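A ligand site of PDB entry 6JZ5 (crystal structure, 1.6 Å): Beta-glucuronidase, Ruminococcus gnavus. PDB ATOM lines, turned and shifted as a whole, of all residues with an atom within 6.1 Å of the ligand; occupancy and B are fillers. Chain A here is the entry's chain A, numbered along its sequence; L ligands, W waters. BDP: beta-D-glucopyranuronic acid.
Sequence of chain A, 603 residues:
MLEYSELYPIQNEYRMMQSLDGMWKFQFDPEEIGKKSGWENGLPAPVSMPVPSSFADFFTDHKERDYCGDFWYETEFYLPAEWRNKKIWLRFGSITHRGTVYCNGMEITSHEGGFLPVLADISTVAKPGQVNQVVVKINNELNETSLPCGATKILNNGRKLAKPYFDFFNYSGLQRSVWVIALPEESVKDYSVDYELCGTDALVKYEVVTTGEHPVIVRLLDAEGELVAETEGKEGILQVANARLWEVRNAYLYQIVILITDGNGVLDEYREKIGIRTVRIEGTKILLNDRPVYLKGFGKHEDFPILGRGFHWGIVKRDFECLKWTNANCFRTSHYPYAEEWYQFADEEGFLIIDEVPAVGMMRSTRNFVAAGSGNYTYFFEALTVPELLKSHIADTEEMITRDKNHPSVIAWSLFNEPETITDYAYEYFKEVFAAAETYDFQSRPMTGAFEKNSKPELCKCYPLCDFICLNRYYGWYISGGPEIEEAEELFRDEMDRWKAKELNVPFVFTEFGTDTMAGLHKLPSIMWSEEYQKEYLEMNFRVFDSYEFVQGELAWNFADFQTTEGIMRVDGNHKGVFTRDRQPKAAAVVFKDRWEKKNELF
O1 of the ligand is in hydrogen-bond range of OE2 of Glu 418.
The side-chain hydroxyl (OH) of Tyr 478 is in hydrogen-bond range of an oxygen (O6B) of the ligand.
An oxygen (O4) of the ligand lies within hydrogen-bond range of the side-chain carboxylate (OD2) of Asp 167, 2.6 Å away.
A ring nitrogen (NE2) of His 335 lies within hydrogen-bond range of an oxygen (O3) of the ligand (2.7 Å).
O2 of the ligand lies within hydrogen-bond range of OE2 of Glu 512, at 2.7 Å.
The side-chain amino group (NZ) of Lys 576 lies within salt-bridge range of an oxygen (O6A) of the ligand.
O2 of the ligand is in hydrogen-bond range of ND2 of Asn 417, at 3.0 Å.
NE1 of Trp 557 is in hydrogen-bond range of O4 of the ligand.
The side-chain amide nitrogen (ND2) of Asn 574 lies within hydrogen-bond range of an oxygen (O6A) of the ligand (3.1 Å).
O6B of the ligand lies within salt-bridge range of NH2 of Arg 570.
OH of Tyr 478 is in hydrogen-bond range of NZ of Lys 576, 2.9 Å away.
OD2 of Asp 167 lies within hydrogen-bond range of ND2 of Asn 574, 2.9 Å away.
OD1 of Asp 167 is in salt-bridge range of NE of Arg 570, 3.0 Å away.
OH of Tyr 474 is in hydrogen-bond range of OE1 of Glu 512 (2.6 Å).
The side-chain carboxylate (OD2) of Asp 516 is in salt-bridge range of the side-chain amino group (NZ) of Lys 576 (2.7 Å).
The side-chain amide nitrogen (ND2) of Asn 472 sits at hydrogen-bond distance from the side-chain amide oxygen (OD1) of Asn 417.
The side-chain amide oxygen (OD1) of Asn 417 sits at hydrogen-bond distance from the guanidinium group (NH1) of Arg 332, at 2.9 Å.
The backbone NH (N) of Asn 574 sits at hydrogen-bond distance from the backbone carbonyl oxygen (O) of Phe 562 (2.8 Å).
Residues that only touch the ligand: Asn 472, Tyr 474 and Phe 562.
Hydrophobic or aromatic side chains that line the ligand: His 335, Tyr 474, Tyr 478, Trp 557 and Phe 562.
Water W5 lies within hydrogen-bond range of an oxygen (O3) of the ligand (2.8 Å), the backbone carbonyl oxygen (O) of Asp 167 (2.9 Å) and a ring nitrogen (NE2) of His 301 (2.9 Å).
Water W2 lies within hydrogen-bond range of the side-chain carboxylate of Glu 418 (2.6 Å) and an oxygen (O1) of the ligand (2.9 Å).
Water W4 bridges an oxygen (O3) of the ligand and the backbone NH (N) of Asp 167.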
ATOM      1  N   ASP A 167      -9.096  -5.718  30.956  1.00  0.00           N
ATOM      2  CA  ASP A 167      -7.720  -6.192  30.920  1.00  0.00           C
ATOM      3  C   ASP A 167      -6.715  -5.138  31.391  1.00  0.00           C
ATOM      4  O   ASP A 167      -5.788  -4.770  30.671  1.00  0.00           O
ATOM      5  CB  ASP A 167      -7.395  -6.649  29.480  1.00  0.00           C
ATOM      6  CG  ASP A 167      -6.052  -7.343  29.353  1.00  0.00           C
ATOM      7  OD1 ASP A 167      -5.648  -8.065  30.298  1.00  0.00           O
ATOM      8  OD2 ASP A 167      -5.402  -7.170  28.305  1.00  0.00           O
ATOM      9  N   PHE A 168      -6.907  -4.606  32.595  1.00  0.00           N
ATOM     10  CA  PHE A 168      -5.848  -3.784  33.192  1.00  0.00           C
ATOM     11  C   PHE A 168      -5.972  -3.849  34.705  1.00  0.00           C
ATOM     12  O   PHE A 168      -7.063  -4.084  35.239  1.00  0.00           O
ATOM     13  CB  PHE A 168      -5.850  -2.310  32.654  1.00  0.00           C
ATOM     14  CG  PHE A 168      -7.202  -1.602  32.668  1.00  0.00           C
ATOM     15  CD1 PHE A 168      -7.561  -0.773  33.723  1.00  0.00           C
ATOM     16  CD2 PHE A 168      -8.065  -1.696  31.575  1.00  0.00           C
ATOM     17  CE1 PHE A 168      -8.770  -0.076  33.703  1.00  0.00           C
ATOM     18  CE2 PHE A 168      -9.282  -1.015  31.548  1.00  0.00           C
ATOM     19  CZ  PHE A 168      -9.635  -0.207  32.617  1.00  0.00           C
ATOM     20  N   HIS A 301      -1.876   3.722  28.151  1.00  0.00           N
ATOM     21  CA  HIS A 301      -2.454   3.544  29.477  1.00  0.00           C
ATOM     22  C   HIS A 301      -1.748   4.563  30.351  1.00  0.00           C
ATOM     23  O   HIS A 301      -0.689   5.057  29.982  1.00  0.00           O
ATOM     24  CB  HIS A 301      -2.220   2.113  30.032  1.00  0.00           C
ATOM     25  CG  HIS A 301      -3.412   1.199  29.892  1.00  0.00           C
ATOM     26  ND1 HIS A 301      -4.578   1.381  30.607  1.00  0.00           N
ATOM     27  CD2 HIS A 301      -3.601   0.094  29.117  1.00  0.00           C
ATOM     28  CE1 HIS A 301      -5.444   0.433  30.262  1.00  0.00           C
ATOM     29  NE2 HIS A 301      -4.876  -0.355  29.375  1.00  0.00           N
ATOM     30  N   ARG A 332      -5.234   7.323  21.603  1.00  0.00           N
ATOM     31  CA  ARG A 332      -6.522   7.200  22.282  1.00  0.00           C
ATOM     32  C   ARG A 332      -6.268   7.070  23.780  1.00  0.00           C
ATOM     33  O   ARG A 332      -5.329   6.395  24.173  1.00  0.00           O
ATOM     34  CB  ARG A 332      -7.307   5.987  21.755  1.00  0.00           C
ATOM     35  CG  ARG A 332      -8.590   5.718  22.525  1.00  0.00           C
ATOM     36  CD  ARG A 332      -9.417   4.588  21.904  1.00  0.00           C
ATOM     37  NE  ARG A 332      -8.669   3.324  21.839  1.00  0.00           N
ATOM     38  CZ  ARG A 332      -9.142   2.145  22.234  1.00  0.00           C
ATOM     39  NH1 ARG A 332     -10.355   2.043  22.766  1.00  0.00           N
ATOM     40  NH2 ARG A 332      -8.377   1.065  22.104  1.00  0.00           N
ATOM     41  N   HIS A 335      -8.225   3.242  28.796  1.00  0.00           N
ATOM     42  CA  HIS A 335      -9.672   3.182  28.564  1.00  0.00           C
ATOM     43  C   HIS A 335     -10.363   4.036  29.616  1.00  0.00           C
ATOM     44  O   HIS A 335     -11.226   3.545  30.356  1.00  0.00           O
ATOM     45  CB  HIS A 335     -10.210   1.750  28.692  1.00  0.00           C
ATOM     46  CG  HIS A 335      -9.707   0.810  27.646  1.00  0.00           C
ATOM     47  ND1 HIS A 335      -9.976   0.982  26.298  1.00  0.00           N
ATOM     48  CD2 HIS A 335      -8.982  -0.329  27.744  1.00  0.00           C
ATOM     49  CE1 HIS A 335      -9.436  -0.015  25.617  1.00  0.00           C
ATOM     50  NE2 HIS A 335      -8.838  -0.832  26.468  1.00  0.00           N
ATOM     51  N   VAL A 360     -15.810   0.306  29.801  1.00  0.00           N
ATOM     52  CA  VAL A 360     -15.194  -0.948  29.432  1.00  0.00           C
ATOM     53  C   VAL A 360     -15.656  -1.985  30.441  1.00  0.00           C
ATOM     54  O   VAL A 360     -15.913  -1.644  31.611  1.00  0.00           O
ATOM     55  CB  VAL A 360     -13.651  -0.831  29.400  1.00  0.00           C
ATOM     56  CG1 VAL A 360     -13.111  -0.504  30.793  1.00  0.00           C
ATOM     57  CG2 VAL A 360     -13.011  -2.075  28.827  1.00  0.00           C
ATOM     58  N   ASN A 417     -15.777   0.874  24.841  1.00  0.00           N
ATOM     59  CA  ASN A 417     -14.809  -0.077  24.310  1.00  0.00           C
ATOM     60  C   ASN A 417     -15.345  -1.487  24.501  1.00  0.00           C
ATOM     61  O   ASN A 417     -15.359  -2.012  25.628  1.00  0.00           O
ATOM     62  CB  ASN A 417     -13.445   0.098  24.986  1.00  0.00           C
ATOM     63  CG  ASN A 417     -12.381  -0.834  24.404  1.00  0.00           C
ATOM     64  OD1 ASN A 417     -11.686  -0.472  23.454  1.00  0.00           O
ATOM     65  ND2 ASN A 417     -12.246  -2.015  24.994  1.00  0.00           N
ATOM     66  N   GLU A 418     -15.828  -2.059  23.414  1.00  0.00           N
ATOM     67  CA  GLU A 418     -16.244  -3.457  23.332  1.00  0.00           C
ATOM     68  C   GLU A 418     -17.377  -3.838  24.286  1.00  0.00           C
ATOM     69  O   GLU A 418     -17.246  -4.766  25.081  1.00  0.00           O
ATOM     70  CB  GLU A 418     -15.043  -4.384  23.582  1.00  0.00           C
ATOM     71  CG  GLU A 418     -13.965  -4.281  22.502  1.00  0.00           C
ATOM     72  CD  GLU A 418     -12.809  -5.218  22.772  1.00  0.00           C
ATOM     73  OE1 GLU A 418     -12.867  -5.967  23.773  1.00  0.00           O
ATOM     74  OE2 GLU A 418     -11.815  -5.192  21.991  1.00  0.00           O
ATOM     75  N   GLU A 452     -15.601  -4.625  19.430  1.00  0.00           N
ATOM     76  CA  GLU A 452     -15.026  -5.970  19.340  1.00  0.00           C
ATOM     77  C   GLU A 452     -15.670  -6.779  18.215  1.00  0.00           C
ATOM     78  O   GLU A 452     -16.730  -6.406  17.690  1.00  0.00           O
ATOM     79  CB  GLU A 452     -15.176  -6.701  20.680  1.00  0.00           C
ATOM     80  CG  GLU A 452     -14.630  -8.116  20.682  1.00  0.00           C
ATOM     81  CD  GLU A 452     -15.092  -8.908  21.882  1.00  0.00           C
ATOM     82  OE1 GLU A 452     -15.885  -8.357  22.691  1.00  0.00           O
ATOM     83  OE2 GLU A 452     -14.664 -10.071  22.028  1.00  0.00           O
ATOM     84  N   ASN A 472     -11.513  -2.887  17.069  1.00  0.00           N
ATOM     85  CA  ASN A 472     -10.433  -3.624  17.710  1.00  0.00           C
ATOM     86  C   ASN A 472     -10.326  -5.008  17.084  1.00  0.00           C
ATOM     87  O   ASN A 472     -11.289  -5.773  17.148  1.00  0.00           O
ATOM     88  CB  ASN A 472     -10.687  -3.785  19.211  1.00  0.00           C
ATOM     89  CG  ASN A 472     -10.710  -2.461  19.970  1.00  0.00           C
ATOM     90  OD1 ASN A 472     -10.359  -1.396  19.446  1.00  0.00           O
ATOM     91  ND2 ASN A 472     -11.126  -2.526  21.226  1.00  0.00           N
ATOM     92  N   TYR A 474      -7.859  -8.673  16.290  1.00  0.00           N
ATOM     93  CA  TYR A 474      -6.705  -9.494  16.630  1.00  0.00           C
ATOM     94  C   TYR A 474      -6.597 -10.719  15.724  1.00  0.00           C
ATOM     95  O   TYR A 474      -6.291 -11.834  16.170  1.00  0.00           O
ATOM     96  CB  TYR A 474      -6.767  -9.875  18.114  1.00  0.00           C
ATOM     97  CG  TYR A 474      -6.543  -8.668  19.006  1.00  0.00           C
ATOM     98  CD1 TYR A 474      -5.250  -8.226  19.278  1.00  0.00           C
ATOM     99  CD2 TYR A 474      -7.614  -7.955  19.518  1.00  0.00           C
ATOM    100  CE1 TYR A 474      -5.038  -7.127  20.070  1.00  0.00           C
ATOM    101  CE2 TYR A 474      -7.393  -6.839  20.317  1.00  0.00           C
ATOM    102  CZ  TYR A 474      -6.103  -6.434  20.595  1.00  0.00           C
ATOM    103  OH  TYR A 474      -5.864  -5.326  21.390  1.00  0.00           O
ATOM    104  N   TYR A 478      -5.507 -13.628  18.586  1.00  0.00           N
ATOM    105  CA  TYR A 478      -6.565 -14.428  19.216  1.00  0.00           C
ATOM    106  C   TYR A 478      -7.297 -15.296  18.201  1.00  0.00           C
ATOM    107  O   TYR A 478      -7.879 -16.325  18.568  1.00  0.00           O
ATOM    108  CB  TYR A 478      -7.566 -13.520  19.927  1.00  0.00           C
ATOM    109  CG  TYR A 478      -7.012 -12.824  21.150  1.00  0.00           C
ATOM    110  CD1 TYR A 478      -6.404 -13.547  22.170  1.00  0.00           C
ATOM    111  CD2 TYR A 478      -7.086 -11.439  21.285  1.00  0.00           C
ATOM    112  CE1 TYR A 478      -5.896 -12.925  23.278  1.00  0.00           C
ATOM    113  CE2 TYR A 478      -6.575 -10.805  22.387  1.00  0.00           C
ATOM    114  CZ  TYR A 478      -5.979 -11.549  23.388  1.00  0.00           C
ATOM    115  OH  TYR A 478      -5.481 -10.919  24.488  1.00  0.00           O
ATOM    116  N   GLU A 512      -7.302  -0.973  17.843  1.00  0.00           N
ATOM    117  CA  GLU A 512      -6.421  -1.969  18.461  1.00  0.00           C
ATOM    118  C   GLU A 512      -6.053  -3.061  17.488  1.00  0.00           C
ATOM    119  O   GLU A 512      -6.884  -3.521  16.706  1.00  0.00           O
ATOM    120  CB  GLU A 512      -7.071  -2.622  19.697  1.00  0.00           C
ATOM    121  CG  GLU A 512      -7.371  -1.639  20.827  1.00  0.00           C
ATOM    122  CD  GLU A 512      -7.848  -2.320  22.097  1.00  0.00           C
ATOM    123  OE1 GLU A 512      -7.583  -3.523  22.279  1.00  0.00           O
ATOM    124  OE2 GLU A 512      -8.499  -1.644  22.919  1.00  0.00           O
ATOM    125  N   ASP A 516       1.121 -10.216  21.978  1.00  0.00           N
ATOM    126  CA  ASP A 516       2.002 -10.193  23.137  1.00  0.00           C
ATOM    127  C   ASP A 516       3.385 -10.544  22.665  1.00  0.00           C
ATOM    128  O   ASP A 516       3.568 -11.458  21.865  1.00  0.00           O
ATOM    129  CB  ASP A 516       1.554 -11.166  24.238  1.00  0.00           C
ATOM    130  CG  ASP A 516       0.388 -10.624  25.030  1.00  0.00           C
ATOM    131  OD1 ASP A 516       0.623 -10.103  26.142  1.00  0.00           O
ATOM    132  OD2 ASP A 516      -0.754 -10.704  24.524  1.00  0.00           O
ATOM    133  N   TRP A 557      -2.216  -1.466  19.474  1.00  0.00           N
ATOM    134  CA  TRP A 557      -2.321  -1.854  20.881  1.00  0.00           C
ATOM    135  C   TRP A 557      -1.064  -2.617  21.273  1.00  0.00           C
ATOM    136  O   TRP A 557      -0.803  -3.655  20.656  1.00  0.00           O
ATOM    137  CB  TRP A 557      -3.542  -2.743  21.101  1.00  0.00           C
ATOM    138  CG  TRP A 557      -3.892  -2.917  22.547  1.00  0.00           C
ATOM    139  CD1 TRP A 557      -3.785  -4.064  23.294  1.00  0.00           C
ATOM    140  CD2 TRP A 557      -4.407  -1.915  23.424  1.00  0.00           C
ATOM    141  NE1 TRP A 557      -4.212  -3.827  24.581  1.00  0.00           N
ATOM    142  CE2 TRP A 557      -4.597  -2.514  24.692  1.00  0.00           C
ATOM    143  CE3 TRP A 557      -4.723  -0.554  23.268  1.00  0.00           C
ATOM    144  CZ2 TRP A 557      -5.101  -1.814  25.777  1.00  0.00           C
ATOM    145  CZ3 TRP A 557      -5.227   0.146  24.353  1.00  0.00           C
ATOM    146  CH2 TRP A 557      -5.412  -0.486  25.606  1.00  0.00           C
ATOM    147  N   PHE A 562       2.011  -3.059  29.907  1.00  0.00           N
ATOM    148  CA  PHE A 562       1.317  -2.477  31.050  1.00  0.00           C
ATOM    149  C   PHE A 562       0.747  -3.549  31.985  1.00  0.00           C
ATOM    150  O   PHE A 562       0.570  -4.708  31.600  1.00  0.00           O
ATOM    151  CB  PHE A 562       0.198  -1.543  30.560  1.00  0.00           C
ATOM    152  CG  PHE A 562      -0.887  -2.238  29.767  1.00  0.00           C
ATOM    153  CD1 PHE A 562      -1.987  -2.795  30.405  1.00  0.00           C
ATOM    154  CD2 PHE A 562      -0.811  -2.305  28.375  1.00  0.00           C
ATOM    155  CE1 PHE A 562      -2.997  -3.429  29.689  1.00  0.00           C
ATOM    156  CE2 PHE A 562      -1.830  -2.948  27.634  1.00  0.00           C
ATOM    157  CZ  PHE A 562      -2.924  -3.508  28.303  1.00  0.00           C
ATOM    158  N   ARG A 570      -1.437 -13.869  31.222  1.00  0.00           N
ATOM    159  CA  ARG A 570      -0.732 -12.597  31.344  1.00  0.00           C
ATOM    160  C   ARG A 570       0.595 -12.796  32.048  1.00  0.00           C
ATOM    161  O   ARG A 570       0.646 -13.099  33.255  1.00  0.00           O
ATOM    162  CB  ARG A 570      -1.602 -11.577  32.084  1.00  0.00           C
ATOM    163  CG  ARG A 570      -2.824 -11.114  31.269  1.00  0.00           C
ATOM    164  CD  ARG A 570      -2.376 -10.178  30.141  1.00  0.00           C
ATOM    165  NE  ARG A 570      -3.468  -9.760  29.245  1.00  0.00           N
ATOM    166  CZ  ARG A 570      -3.772 -10.378  28.107  1.00  0.00           C
ATOM    167  NH1 ARG A 570      -3.117 -11.488  27.743  1.00  0.00           N
ATOM    168  NH2 ARG A 570      -4.746  -9.904  27.338  1.00  0.00           N
ATOM    169  N   ASN A 574       0.317  -7.238  30.398  1.00  0.00           N
ATOM    170  CA  ASN A 574       0.043  -7.308  28.980  1.00  0.00           C
ATOM    171  C   ASN A 574       1.293  -6.906  28.214  1.00  0.00           C
ATOM    172  O   ASN A 574       1.855  -5.834  28.454  1.00  0.00           O
ATOM    173  CB  ASN A 574      -1.146  -6.394  28.659  1.00  0.00           C
ATOM    174  CG  ASN A 574      -1.595  -6.492  27.205  1.00  0.00           C
ATOM    175  OD1 ASN A 574      -0.794  -6.289  26.281  1.00  0.00           O
ATOM    176  ND2 ASN A 574      -2.879  -6.786  26.996  1.00  0.00           N
ATOM    177  N   LYS A 576       1.634  -6.620  24.826  1.00  0.00           N
ATOM    178  CA  LYS A 576       1.388  -6.168  23.464  1.00  0.00           C
ATOM    179  C   LYS A 576       2.040  -4.804  23.182  1.00  0.00           C
ATOM    180  O   LYS A 576       1.879  -4.241  22.092  1.00  0.00           O
ATOM    181  CB  LYS A 576      -0.111  -6.109  23.177  1.00  0.00           C
ATOM    182  CG  LYS A 576      -0.782  -7.478  23.285  1.00  0.00           C
ATOM    183  CD  LYS A 576      -2.160  -7.493  22.644  1.00  0.00           C
ATOM    184  CE  LYS A 576      -2.766  -8.910  22.641  1.00  0.00           C
ATOM    185  NZ  LYS A 576      -3.068  -9.393  24.029  1.00  0.00           N
HETATM  186  C1  BDP L   1      -9.017  -5.767  23.817  1.00  0.00           C
HETATM  187  C2  BDP L   1      -9.171  -4.696  24.900  1.00  0.00           C
HETATM  188  C3  BDP L   1      -7.875  -4.354  25.509  1.00  0.00           C
HETATM  189  C4  BDP L   1      -7.097  -5.534  25.913  1.00  0.00           C
HETATM  190  C5  BDP L   1      -6.916  -6.430  24.686  1.00  0.00           C
HETATM  191  C6  BDP L   1      -6.027  -7.594  24.819  1.00  0.00           C
HETATM  192  O2  BDP L   1      -9.758  -3.558  24.392  1.00  0.00           O
HETATM  193  O3  BDP L   1      -8.067  -3.403  26.587  1.00  0.00           O
HETATM  194  O4  BDP L   1      -5.877  -5.366  26.551  1.00  0.00           O
HETATM  195  O5  BDP L   1      -8.202  -6.884  24.224  1.00  0.00           O
HETATM  196  O6A BDP L   1      -4.869  -7.430  24.707  1.00  0.00           O
HETATM  197  O1  BDP L   1     -10.292  -6.310  23.567  1.00  0.00           O
HETATM  198  O6B BDP L   1      -6.562  -8.680  25.060  1.00  0.00           O
HETATM  199  O   HOH W   1      -9.269  -9.193  24.628  1.00  0.00           O
HETATM  200  O   HOH W   2     -11.076  -7.519  20.997  1.00  0.00           O
HETATM  201  O   HOH W   3      -8.544  -8.938  27.014  1.00  0.00           O
HETATM  202  O   HOH W   4     -10.347  -4.182  28.465  1.00  0.00           O
HETATM  203  O   HOH W   5      -6.431  -2.732  28.775  1.00  0.00           O
